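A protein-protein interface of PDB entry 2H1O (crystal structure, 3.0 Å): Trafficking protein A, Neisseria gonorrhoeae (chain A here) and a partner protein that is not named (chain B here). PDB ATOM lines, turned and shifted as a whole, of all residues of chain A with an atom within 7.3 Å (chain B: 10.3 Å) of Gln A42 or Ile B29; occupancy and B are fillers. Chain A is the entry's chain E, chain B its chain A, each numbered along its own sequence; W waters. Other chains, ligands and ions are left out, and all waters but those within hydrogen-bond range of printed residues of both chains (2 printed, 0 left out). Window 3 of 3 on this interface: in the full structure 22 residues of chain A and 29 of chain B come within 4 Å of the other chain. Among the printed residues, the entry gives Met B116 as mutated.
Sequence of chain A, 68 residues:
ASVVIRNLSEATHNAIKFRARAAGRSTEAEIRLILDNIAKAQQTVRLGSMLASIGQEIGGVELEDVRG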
ATOM      1  N   ASP A  36      -3.728  34.490  -4.845  1.00  0.00           N
ATOM      2  CA  ASP A  36      -3.507  33.737  -3.625  1.00  0.00           C
ATOM      3  C   ASP A  36      -4.238  32.390  -3.673  1.00  0.00           C
ATOM      4  O   ASP A  36      -3.729  31.381  -3.203  1.00  0.00           O
ATOM      5  CB  ASP A  36      -3.969  34.569  -2.422  1.00  0.00           C
ATOM      6  CG  ASP A  36      -2.796  35.166  -1.631  1.00  0.00           C
ATOM      7  OD1 ASP A  36      -2.173  34.400  -0.859  1.00  0.00           O
ATOM      8  OD2 ASP A  36      -2.481  36.380  -1.776  1.00  0.00           O
ATOM      9  N   ASN A  37      -5.422  32.365  -4.270  1.00  0.00           N
ATOM     10  CA  ASN A  37      -6.188  31.126  -4.348  1.00  0.00           C
ATOM     11  C   ASN A  37      -5.521  30.020  -5.157  1.00  0.00           C
ATOM     12  O   ASN A  37      -5.463  28.878  -4.712  1.00  0.00           O
ATOM     13  CB  ASN A  37      -7.586  31.407  -4.900  1.00  0.00           C
ATOM     14  CG  ASN A  37      -8.554  31.880  -3.824  1.00  0.00           C
ATOM     15  OD1 ASN A  37      -9.479  32.645  -4.100  1.00  0.00           O
ATOM     16  ND2 ASN A  37      -8.357  31.413  -2.599  1.00  0.00           N
ATOM     17  N   ILE A  38      -5.012  30.339  -6.337  1.00  0.00           N
ATOM     18  CA  ILE A  38      -4.370  29.310  -7.135  1.00  0.00           C
ATOM     19  C   ILE A  38      -3.039  28.923  -6.501  1.00  0.00           C
ATOM     20  O   ILE A  38      -2.593  27.778  -6.605  1.00  0.00           O
ATOM     21  CB  ILE A  38      -4.121  29.785  -8.563  1.00  0.00           C
ATOM     22  CG1 ILE A  38      -2.996  30.805  -8.578  1.00  0.00           C
ATOM     23  CG2 ILE A  38      -5.384  30.407  -9.131  1.00  0.00           C
ATOM     24  CD1 ILE A  38      -2.721  31.319  -9.950  1.00  0.00           C
ATOM     25  N   ALA A  39      -2.408  29.886  -5.836  1.00  0.00           N
ATOM     26  CA  ALA A  39      -1.130  29.638  -5.180  1.00  0.00           C
ATOM     27  C   ALA A  39      -1.307  28.550  -4.138  1.00  0.00           C
ATOM     28  O   ALA A  39      -0.535  27.601  -4.091  1.00  0.00           O
ATOM     29  CB  ALA A  39      -0.619  30.909  -4.529  1.00  0.00           C
ATOM     30  N   LYS A  40      -2.337  28.691  -3.310  1.00  0.00           N
ATOM     31  CA  LYS A  40      -2.633  27.722  -2.259  1.00  0.00           C
ATOM     32  C   LYS A  40      -2.922  26.367  -2.885  1.00  0.00           C
ATOM     33  O   LYS A  40      -2.786  25.321  -2.240  1.00  0.00           O
ATOM     34  CB  LYS A  40      -3.848  28.173  -1.447  1.00  0.00           C
ATOM     35  CG  LYS A  40      -3.977  27.521  -0.067  1.00  0.00           C
ATOM     36  CD  LYS A  40      -5.393  26.975   0.180  1.00  0.00           C
ATOM     37  CE  LYS A  40      -6.498  27.918  -0.353  1.00  0.00           C
ATOM     38  NZ  LYS A  40      -6.479  29.311   0.209  1.00  0.00           N
ATOM     39  N   ALA A  41      -3.335  26.396  -4.145  1.00  0.00           N
ATOM     40  CA  ALA A  41      -3.617  25.178  -4.873  1.00  0.00           C
ATOM     41  C   ALA A  41      -2.283  24.506  -5.229  1.00  0.00           C
ATOM     42  O   ALA A  41      -2.140  23.291  -5.094  1.00  0.00           O
ATOM     43  CB  ALA A  41      -4.405  25.503  -6.115  1.00  0.00           C
ATOM     44  N   GLN A  42      -1.302  25.294  -5.673  1.00  0.00           N
ATOM     45  CA  GLN A  42       0.017  24.752  -6.010  1.00  0.00           C
ATOM     46  C   GLN A  42       0.682  24.155  -4.769  1.00  0.00           C
ATOM     47  O   GLN A  42       1.505  23.248  -4.867  1.00  0.00           O
ATOM     48  CB  GLN A  42       0.939  25.844  -6.565  1.00  0.00           C
ATOM     49  CG  GLN A  42       0.689  26.268  -8.006  1.00  0.00           C
ATOM     50  CD  GLN A  42       1.186  25.262  -9.045  1.00  0.00           C
ATOM     51  OE1 GLN A  42       2.381  24.960  -9.128  1.00  0.00           O
ATOM     52  NE2 GLN A  42       0.263  24.750  -9.851  1.00  0.00           N
ATOM     53  N   GLN A  43       0.331  24.687  -3.605  1.00  0.00           N
ATOM     54  CA  GLN A  43       0.892  24.234  -2.339  1.00  0.00           C
ATOM     55  C   GLN A  43       0.447  22.816  -2.011  1.00  0.00           C
ATOM     56  O   GLN A  43      -0.483  22.617  -1.225  1.00  0.00           O
ATOM     57  CB  GLN A  43       0.447  25.169  -1.210  1.00  0.00           C
ATOM     58  CG  GLN A  43       1.227  25.035   0.097  1.00  0.00           C
ATOM     59  CD  GLN A  43       2.591  25.689   0.020  1.00  0.00           C
ATOM     60  OE1 GLN A  43       3.263  25.877   1.030  1.00  0.00           O
ATOM     61  NE2 GLN A  43       3.007  26.039  -1.188  1.00  0.00           N
ATOM     62  N   THR A  44       1.110  21.834  -2.611  1.00  0.00           N
ATOM     63  CA  THR A  44       0.777  20.437  -2.370  1.00  0.00           C
ATOM     64  C   THR A  44       1.245  20.037  -0.976  1.00  0.00           C
ATOM     65  O   THR A  44       0.579  19.277  -0.274  1.00  0.00           O
ATOM     66  CB  THR A  44       1.449  19.518  -3.412  1.00  0.00           C
ATOM     67  OG1 THR A  44       1.009  19.879  -4.727  1.00  0.00           O
ATOM     68  CG2 THR A  44       1.085  18.065  -3.156  1.00  0.00           C
ATOM     69  N   VAL A  45       2.401  20.551  -0.576  1.00  0.00           N
ATOM     70  CA  VAL A  45       2.945  20.246   0.744  1.00  0.00           C
ATOM     71  C   VAL A  45       3.764  21.407   1.303  1.00  0.00           C
ATOM     72  O   VAL A  45       4.363  22.188   0.558  1.00  0.00           O
ATOM     73  CB  VAL A  45       3.808  18.957   0.706  1.00  0.00           C
ATOM     74  CG1 VAL A  45       2.907  17.734   0.662  1.00  0.00           C
ATOM     75  CG2 VAL A  45       4.702  18.965  -0.517  1.00  0.00           C
ATOM     76  N   LEU A  47       6.860  22.040   3.171  1.00  0.00           N
ATOM     77  CA  LEU A  47       8.101  21.442   3.629  1.00  0.00           C
ATOM     78  C   LEU A  47       8.495  21.791   5.060  1.00  0.00           C
ATOM     79  O   LEU A  47       8.827  20.905   5.846  1.00  0.00           O
ATOM     80  CB  LEU A  47       9.229  21.807   2.668  1.00  0.00           C
ATOM     81  CG  LEU A  47      10.429  20.875   2.790  1.00  0.00           C
ATOM     82  CD1 LEU A  47       9.994  19.431   2.521  1.00  0.00           C
ATOM     83  CD2 LEU A  47      11.514  21.318   1.824  1.00  0.00           C
ATOM     84  N   MET B   1      14.769  28.052  -9.398  1.00  0.00           N
ATOM     85  CA  MET B   1      14.583  26.975  -8.389  1.00  0.00           C
ATOM     86  C   MET B   1      15.584  27.183  -7.278  1.00  0.00           C
ATOM     87  O   MET B   1      16.573  27.892  -7.449  1.00  0.00           O
ATOM     88  CB  MET B   1      14.814  25.588  -8.999  1.00  0.00           C
ATOM     89  CG  MET B   1      14.550  25.481 -10.489  1.00  0.00           C
ATOM     90  SD  MET B   1      15.868  26.287 -11.418  1.00  0.00           S
ATOM     91  CE  MET B   1      16.627  24.890 -12.271  1.00  0.00           C
ATOM     92  N   ILE B   2      15.342  26.533  -6.151  1.00  0.00           N
ATOM     93  CA  ILE B   2      16.224  26.673  -5.008  1.00  0.00           C
ATOM     94  C   ILE B   2      16.883  25.364  -4.607  1.00  0.00           C
ATOM     95  O   ILE B   2      16.279  24.296  -4.699  1.00  0.00           O
ATOM     96  CB  ILE B   2      15.457  27.195  -3.790  1.00  0.00           C
ATOM     97  CG1 ILE B   2      14.543  28.340  -4.208  1.00  0.00           C
ATOM     98  CG2 ILE B   2      16.421  27.700  -2.748  1.00  0.00           C
ATOM     99  CD1 ILE B   2      13.616  28.789  -3.112  1.00  0.00           C
ATOM    100  N   LEU B   3      18.124  25.463  -4.143  1.00  0.00           N
ATOM    101  CA  LEU B   3      18.871  24.294  -3.695  1.00  0.00           C
ATOM    102  C   LEU B   3      19.086  24.378  -2.177  1.00  0.00           C
ATOM    103  O   LEU B   3      19.744  25.298  -1.676  1.00  0.00           O
ATOM    104  CB  LEU B   3      20.221  24.233  -4.407  1.00  0.00           C
ATOM    105  CG  LEU B   3      20.959  22.908  -4.309  1.00  0.00           C
ATOM    106  CD1 LEU B   3      20.200  21.855  -5.086  1.00  0.00           C
ATOM    107  CD2 LEU B   3      22.355  23.071  -4.854  1.00  0.00           C
ATOM    108  N   LEU B   4      18.517  23.424  -1.447  1.00  0.00           N
ATOM    109  CA  LEU B   4      18.668  23.415  -0.005  1.00  0.00           C
ATOM    110  C   LEU B   4      19.976  22.780   0.427  1.00  0.00           C
ATOM    111  O   LEU B   4      20.329  21.677   0.015  1.00  0.00           O
ATOM    112  CB  LEU B   4      17.506  22.679   0.662  1.00  0.00           C
ATOM    113  CG  LEU B   4      16.137  23.311   0.464  1.00  0.00           C
ATOM    114  CD1 LEU B   4      15.168  22.719   1.442  1.00  0.00           C
ATOM    115  CD2 LEU B   4      16.229  24.795   0.682  1.00  0.00           C
ATOM    116  N   ALA B  23       9.208  29.054   8.752  1.00  0.00           N
ATOM    117  CA  ALA B  23       8.207  29.875   8.078  1.00  0.00           C
ATOM    118  C   ALA B  23       8.553  29.983   6.599  1.00  0.00           C
ATOM    119  O   ALA B  23       7.692  29.842   5.737  1.00  0.00           O
ATOM    120  CB  ALA B  23       8.157  31.262   8.700  1.00  0.00           C
ATOM    121  N   TRP B  24       9.825  30.224   6.312  1.00  0.00           N
ATOM    122  CA  TRP B  24      10.280  30.344   4.940  1.00  0.00           C
ATOM    123  C   TRP B  24      10.156  29.048   4.129  1.00  0.00           C
ATOM    124  O   TRP B  24       9.867  29.095   2.932  1.00  0.00           O
ATOM    125  CB  TRP B  24      11.725  30.814   4.909  1.00  0.00           C
ATOM    126  CG  TRP B  24      12.242  30.921   3.532  1.00  0.00           C
ATOM    127  CD1 TRP B  24      11.978  31.907   2.633  1.00  0.00           C
ATOM    128  CD2 TRP B  24      13.109  29.992   2.871  1.00  0.00           C
ATOM    129  NE1 TRP B  24      12.629  31.659   1.449  1.00  0.00           N
ATOM    130  CE2 TRP B  24      13.331  30.486   1.566  1.00  0.00           C
ATOM    131  CE3 TRP B  24      13.720  28.787   3.255  1.00  0.00           C
ATOM    132  CZ2 TRP B  24      14.143  29.818   0.640  1.00  0.00           C
ATOM    133  CZ3 TRP B  24      14.525  28.126   2.338  1.00  0.00           C
ATOM    134  CH2 TRP B  24      14.729  28.643   1.045  1.00  0.00           C
ATOM    135  N   LEU B  25      10.393  27.898   4.759  1.00  0.00           N
ATOM    136  CA  LEU B  25      10.276  26.626   4.055  1.00  0.00           C
ATOM    137  C   LEU B  25       8.824  26.390   3.650  1.00  0.00           C
ATOM    138  O   LEU B  25       8.545  25.816   2.596  1.00  0.00           O
ATOM    139  CB  LEU B  25      10.769  25.467   4.928  1.00  0.00           C
ATOM    140  CG  LEU B  25      12.285  25.242   5.047  1.00  0.00           C
ATOM    141  CD1 LEU B  25      12.571  24.284   6.184  1.00  0.00           C
ATOM    142  CD2 LEU B  25      12.840  24.692   3.754  1.00  0.00           C
ATOM    143  N   ASP B  26       7.890  26.840   4.476  1.00  0.00           N
ATOM    144  CA  ASP B  26       6.491  26.653   4.136  1.00  0.00           C
ATOM    145  C   ASP B  26       6.049  27.575   3.023  1.00  0.00           C
ATOM    146  O   ASP B  26       5.106  27.269   2.298  1.00  0.00           O
ATOM    147  CB  ASP B  26       5.604  26.855   5.352  1.00  0.00           C
ATOM    148  CG  ASP B  26       5.690  25.699   6.318  1.00  0.00           C
ATOM    149  OD1 ASP B  26       5.807  24.548   5.846  1.00  0.00           O
ATOM    150  OD2 ASP B  26       5.633  25.932   7.542  1.00  0.00           O
ATOM    151  N   SER B  27       6.728  28.703   2.874  1.00  0.00           N
ATOM    152  CA  SER B  27       6.371  29.627   1.813  1.00  0.00           C
ATOM    153  C   SER B  27       6.946  29.098   0.509  1.00  0.00           C
ATOM    154  O   SER B  27       7.071  29.839  -0.470  1.00  0.00           O
ATOM    155  CB  SER B  27       6.959  31.002   2.077  1.00  0.00           C
ATOM    156  OG  SER B  27       8.338  31.024   1.752  1.00  0.00           O
ATOM    157  N   LEU B  28       7.312  27.821   0.493  1.00  0.00           N
ATOM    158  CA  LEU B  28       7.891  27.244  -0.709  1.00  0.00           C
ATOM    159  C   LEU B  28       6.997  26.216  -1.365  1.00  0.00           C
ATOM    160  O   LEU B  28       6.124  25.636  -0.720  1.00  0.00           O
ATOM    161  CB  LEU B  28       9.240  26.592  -0.403  1.00  0.00           C
ATOM    162  CG  LEU B  28      10.425  27.467  -0.002  1.00  0.00           C
ATOM    163  CD1 LEU B  28      11.657  26.604   0.077  1.00  0.00           C
ATOM    164  CD2 LEU B  28      10.633  28.581  -1.011  1.00  0.00           C
ATOM    165  N   ILE B  29       7.226  26.013  -2.658  1.00  0.00           N
ATOM    166  CA  ILE B  29       6.497  25.034  -3.431  1.00  0.00           C
ATOM    167  C   ILE B  29       7.486  23.914  -3.758  1.00  0.00           C
ATOM    168  O   ILE B  29       8.412  24.096  -4.561  1.00  0.00           O
ATOM    169  CB  ILE B  29       5.948  25.657  -4.718  1.00  0.00           C
ATOM    170  CG1 ILE B  29       4.738  26.519  -4.367  1.00  0.00           C
ATOM    171  CG2 ILE B  29       5.585  24.564  -5.740  1.00  0.00           C
ATOM    172  CD1 ILE B  29       3.988  27.024  -5.555  1.00  0.00           C
ATOM    173  N   LEU B  30       7.273  22.761  -3.122  1.00  0.00           N
ATOM    174  CA  LEU B  30       8.130  21.586  -3.265  1.00  0.00           C
ATOM    175  C   LEU B  30       8.827  21.423  -4.605  1.00  0.00           C
ATOM    176  O   LEU B  30      10.055  21.399  -4.675  1.00  0.00           O
ATOM    177  CB  LEU B  30       7.339  20.315  -2.954  1.00  0.00           C
ATOM    178  CG  LEU B  30       8.216  19.061  -2.816  1.00  0.00           C
ATOM    179  CD1 LEU B  30       9.294  19.291  -1.759  1.00  0.00           C
ATOM    180  CD2 LEU B  30       7.355  17.861  -2.449  1.00  0.00           C
ATOM    181  N   GLU B  31       8.044  21.302  -5.665  1.00  0.00           N
ATOM    182  CA  GLU B  31       8.592  21.134  -7.001  1.00  0.00           C
ATOM    183  C   GLU B  31       9.698  22.130  -7.371  1.00  0.00           C
ATOM    184  O   GLU B  31      10.352  21.972  -8.394  1.00  0.00           O
ATOM    185  CB  GLU B  31       7.464  21.233  -8.018  1.00  0.00           C
ATOM    186  CG  GLU B  31       6.453  20.084  -7.957  1.00  0.00           C
ATOM    187  CD  GLU B  31       5.588  20.074  -6.695  1.00  0.00           C
ATOM    188  OE1 GLU B  31       5.014  21.133  -6.346  1.00  0.00           O
ATOM    189  OE2 GLU B  31       5.466  18.996  -6.062  1.00  0.00           O
ATOM    190  N   ASP B  32       9.918  23.143  -6.539  1.00  0.00           N
ATOM    191  CA  ASP B  32      10.927  24.164  -6.817  1.00  0.00           C
ATOM    192  C   ASP B  32      12.228  23.956  -6.026  1.00  0.00           C
ATOM    193  O   ASP B  32      13.293  24.488  -6.372  1.00  0.00           O
ATOM    194  CB  ASP B  32      10.336  25.533  -6.486  1.00  0.00           C
ATOM    195  CG  ASP B  32      11.115  26.674  -7.110  1.00  0.00           C
ATOM    196  OD1 ASP B  32      12.315  26.828  -6.797  1.00  0.00           O
ATOM    197  OD2 ASP B  32      10.525  27.425  -7.919  1.00  0.00           O
ATOM    198  N   VAL B  33      12.125  23.169  -4.963  1.00  0.00           N
ATOM    199  CA  VAL B  33      13.241  22.888  -4.077  1.00  0.00           C
ATOM    200  C   VAL B  33      13.981  21.634  -4.505  1.00  0.00           C
ATOM    201  O   VAL B  33      13.358  20.615  -4.773  1.00  0.00           O
ATOM    202  CB  VAL B  33      12.724  22.702  -2.637  1.00  0.00           C
ATOM    203  CG1 VAL B  33      13.874  22.404  -1.690  1.00  0.00           C
ATOM    204  CG2 VAL B  33      11.962  23.941  -2.203  1.00  0.00           C
ATOM    205  N   TYR B  34      15.310  21.720  -4.559  1.00  0.00           N
ATOM    206  CA  TYR B  34      16.166  20.593  -4.938  1.00  0.00           C
ATOM    207  C   TYR B  34      17.218  20.320  -3.866  1.00  0.00           C
ATOM    208  O   TYR B  34      17.520  21.185  -3.040  1.00  0.00           O
ATOM    209  CB  TYR B  34      16.907  20.868  -6.258  1.00  0.00           C
ATOM    210  CG  TYR B  34      16.047  20.894  -7.505  1.00  0.00           C
ATOM    211  CD1 TYR B  34      15.183  21.956  -7.755  1.00  0.00           C
ATOM    212  CD2 TYR B  34      16.087  19.847  -8.428  1.00  0.00           C
ATOM    213  CE1 TYR B  34      14.381  21.979  -8.885  1.00  0.00           C
ATOM    214  CE2 TYR B  34      15.286  19.859  -9.560  1.00  0.00           C
ATOM    215  CZ  TYR B  34      14.435  20.930  -9.778  1.00  0.00           C
ATOM    216  OH  TYR B  34      13.619  20.963 -10.880  1.00  0.00           O
ATOM    217  N   LEU B  70      10.075  13.007  -1.234  1.00  0.00           N
ATOM    218  CA  LEU B  70       9.527  14.312  -1.637  1.00  0.00           C
ATOM    219  C   LEU B  70      10.427  15.102  -2.588  1.00  0.00           C
ATOM    220  O   LEU B  70      10.036  16.151  -3.093  1.00  0.00           O
ATOM    221  CB  LEU B  70       9.264  15.178  -0.402  1.00  0.00           C
ATOM    222  CG  LEU B  70       8.077  14.838   0.492  1.00  0.00           C
ATOM    223  CD1 LEU B  70       8.220  15.576   1.809  1.00  0.00           C
ATOM    224  CD2 LEU B  70       6.782  15.208  -0.218  1.00  0.00           C
ATOM    225  N   PHE B  71      11.635  14.609  -2.816  1.00  0.00           N
ATOM    226  CA  PHE B  71      12.552  15.285  -3.702  1.00  0.00           C
ATOM    227  C   PHE B  71      12.930  14.362  -4.846  1.00  0.00           C
ATOM    228  O   PHE B  71      13.921  14.597  -5.538  1.00  0.00           O
ATOM    229  CB  PHE B  71      13.803  15.693  -2.942  1.00  0.00           C
ATOM    230  CG  PHE B  71      13.552  16.684  -1.844  1.00  0.00           C
ATOM    231  CD1 PHE B  71      13.013  16.279  -0.630  1.00  0.00           C
ATOM    232  CD2 PHE B  71      13.901  18.028  -2.009  1.00  0.00           C
ATOM    233  CE1 PHE B  71      12.831  17.194   0.408  1.00  0.00           C
ATOM    234  CE2 PHE B  71      13.723  18.951  -0.982  1.00  0.00           C
ATOM    235  CZ  PHE B  71      13.190  18.534   0.229  1.00  0.00           C
ATOM    236  N   ARG B  74      14.467  15.396  -8.060  1.00  0.00           N
ATOM    237  CA  ARG B  74      15.017  16.715  -7.831  1.00  0.00           C
ATOM    238  C   ARG B  74      16.231  16.626  -6.919  1.00  0.00           C
ATOM    239  O   ARG B  74      16.489  17.519  -6.104  1.00  0.00           O
ATOM    240  CB  ARG B  74      13.959  17.641  -7.240  1.00  0.00           C
ATOM    241  CG  ARG B  74      12.759  17.856  -8.153  1.00  0.00           C
ATOM    242  CD  ARG B  74      11.980  19.102  -7.769  1.00  0.00           C
ATOM    243  NE  ARG B  74      11.685  19.152  -6.334  1.00  0.00           N
ATOM    244  CZ  ARG B  74      10.891  18.301  -5.680  1.00  0.00           C
ATOM    245  NH1 ARG B  74      10.283  17.311  -6.318  1.00  0.00           N
ATOM    246  NH2 ARG B  74      10.720  18.433  -4.370  1.00  0.00           N
ATOM    247  N   MET B 116      20.855  28.028  -9.983  1.00  0.00           N
ATOM    248  CA  MET B 116      19.915  27.974  -8.873  1.00  0.00           C
ATOM    249  C   MET B 116      20.380  28.855  -7.725  1.00  0.00           C
ATOM    250  O   MET B 116      21.509  29.341  -7.713  1.00  0.00           O
ATOM    251  CB  MET B 116      19.799  26.548  -8.359  1.00  0.00           C
ATOM    252  CG  MET B 116      19.392  25.541  -9.401  1.00  0.00           C
ATOM    253  SD  MET B 116      19.342  23.882  -8.708  1.00  0.00           S
ATOM    254  CE  MET B 116      17.748  23.888  -7.926  1.00  0.00           C
HETATM  255  O   HOH W   1       4.884  22.674  -1.850  1.00  0.00           O
HETATM  256  O   HOH W   2       3.843  20.980  -4.025  1.00  0.00           O
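The backbone carbonyl oxygen of Asp B26 lies close to the side-chain amide oxygen of Gln A43 (2.6 Å).
The backbone carbonyl oxygen (O) of Leu B28 is in hydrogen-bond range of the side-chain amide nitrogen (NE2) of Gln A43 (3.2 Å).
The backbone carbonyl oxygen (O) of Leu B30 lies close to the guanidinium group (NH2) of Arg B74 (3.1 Å).
The backbone carbonyl oxygen (O) of Gln A42 sits at hydrogen-bond distance from the side-chain hydroxyl (OG1) of Thr A44, 3.4 Å away.
N of Leu B4 lies within hydrogen-bond range of O of Tyr B34 (2.9 Å).
Among the printed residues, merely in contact across the chains: Gln A42 with Ile B29 (3.4 Å), Val A45 with Leu B30 (3.5 Å), Leu A47 with Phe B71 (3.6 Å), Gln A43 with Ile B29 (3.7 Å), Leu A47 with Asp B26 (3.8 Å) and Leu A47 with Leu B4 (3.9 Å).
No residue of chain B comes within 4 Å of Ala A39.
No residue of chain B comes within 4 Å of Ala A41.
Gln A42 touches one residue of chain B.
Printed residues of chain B within 4 Å of Val A45: Leu B30 (3.5 Å).
Printed residues of chain A within 4 Å of Leu B4: Leu A47 (3.9 Å).
Printed residues of chain A within 4 Å of Asp B26: Gln A43 (2.6 Å) and Leu A47 (3.8 Å).
Of the printed residues of chain A, Leu B28 touches Gln A43.
Ile B29 touches two residues of chain A.
Of the printed residues of chain A, Leu B30 touches Val A45.
The nearest printed residue of chain A that does not touch Leu B4 is Val A45 (10.9 Å).
Of the 20 printed residues of chain B, 6 touch a printed residue of chain A.
Printed residues of chain B that touch a printed residue of chain A: Leu B4, Asp B26, Leu B28, Ile B29, Leu B30 and Phe B71.
Hydrophobic or aromatic side chains of chain B that line the printed part of chain A: Leu B4, Ile B29, Leu B30 and Phe B71.
Of the 11 printed residues of chain A, 4 touch a printed residue of chain B.
Printed residues of chain A that touch a printed residue of chain B: Gln A42, Gln A43, Val A45 and Leu A47.
Hydrophobic or aromatic side chains of chain A within 4 Å of the printed part of chain B: Val A45 and Leu A47.
Among the printed residues, no Asp or Glu carboxylate lies within 4 Å of a Lys or Arg side-chain nitrogen of the other chain.
Water W1 lies within hydrogen-bond range of O of Val A45 (2.5 Å), N of Leu B30 (2.7 Å) and O of Leu B28 (3.4 Å).
Water W2 lies within hydrogen-bond range of OE1 of Glu B31 (2.6 Å), OG1 of Thr A44 (3.1 Å) and O of Gln A42 (3.4 Å).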
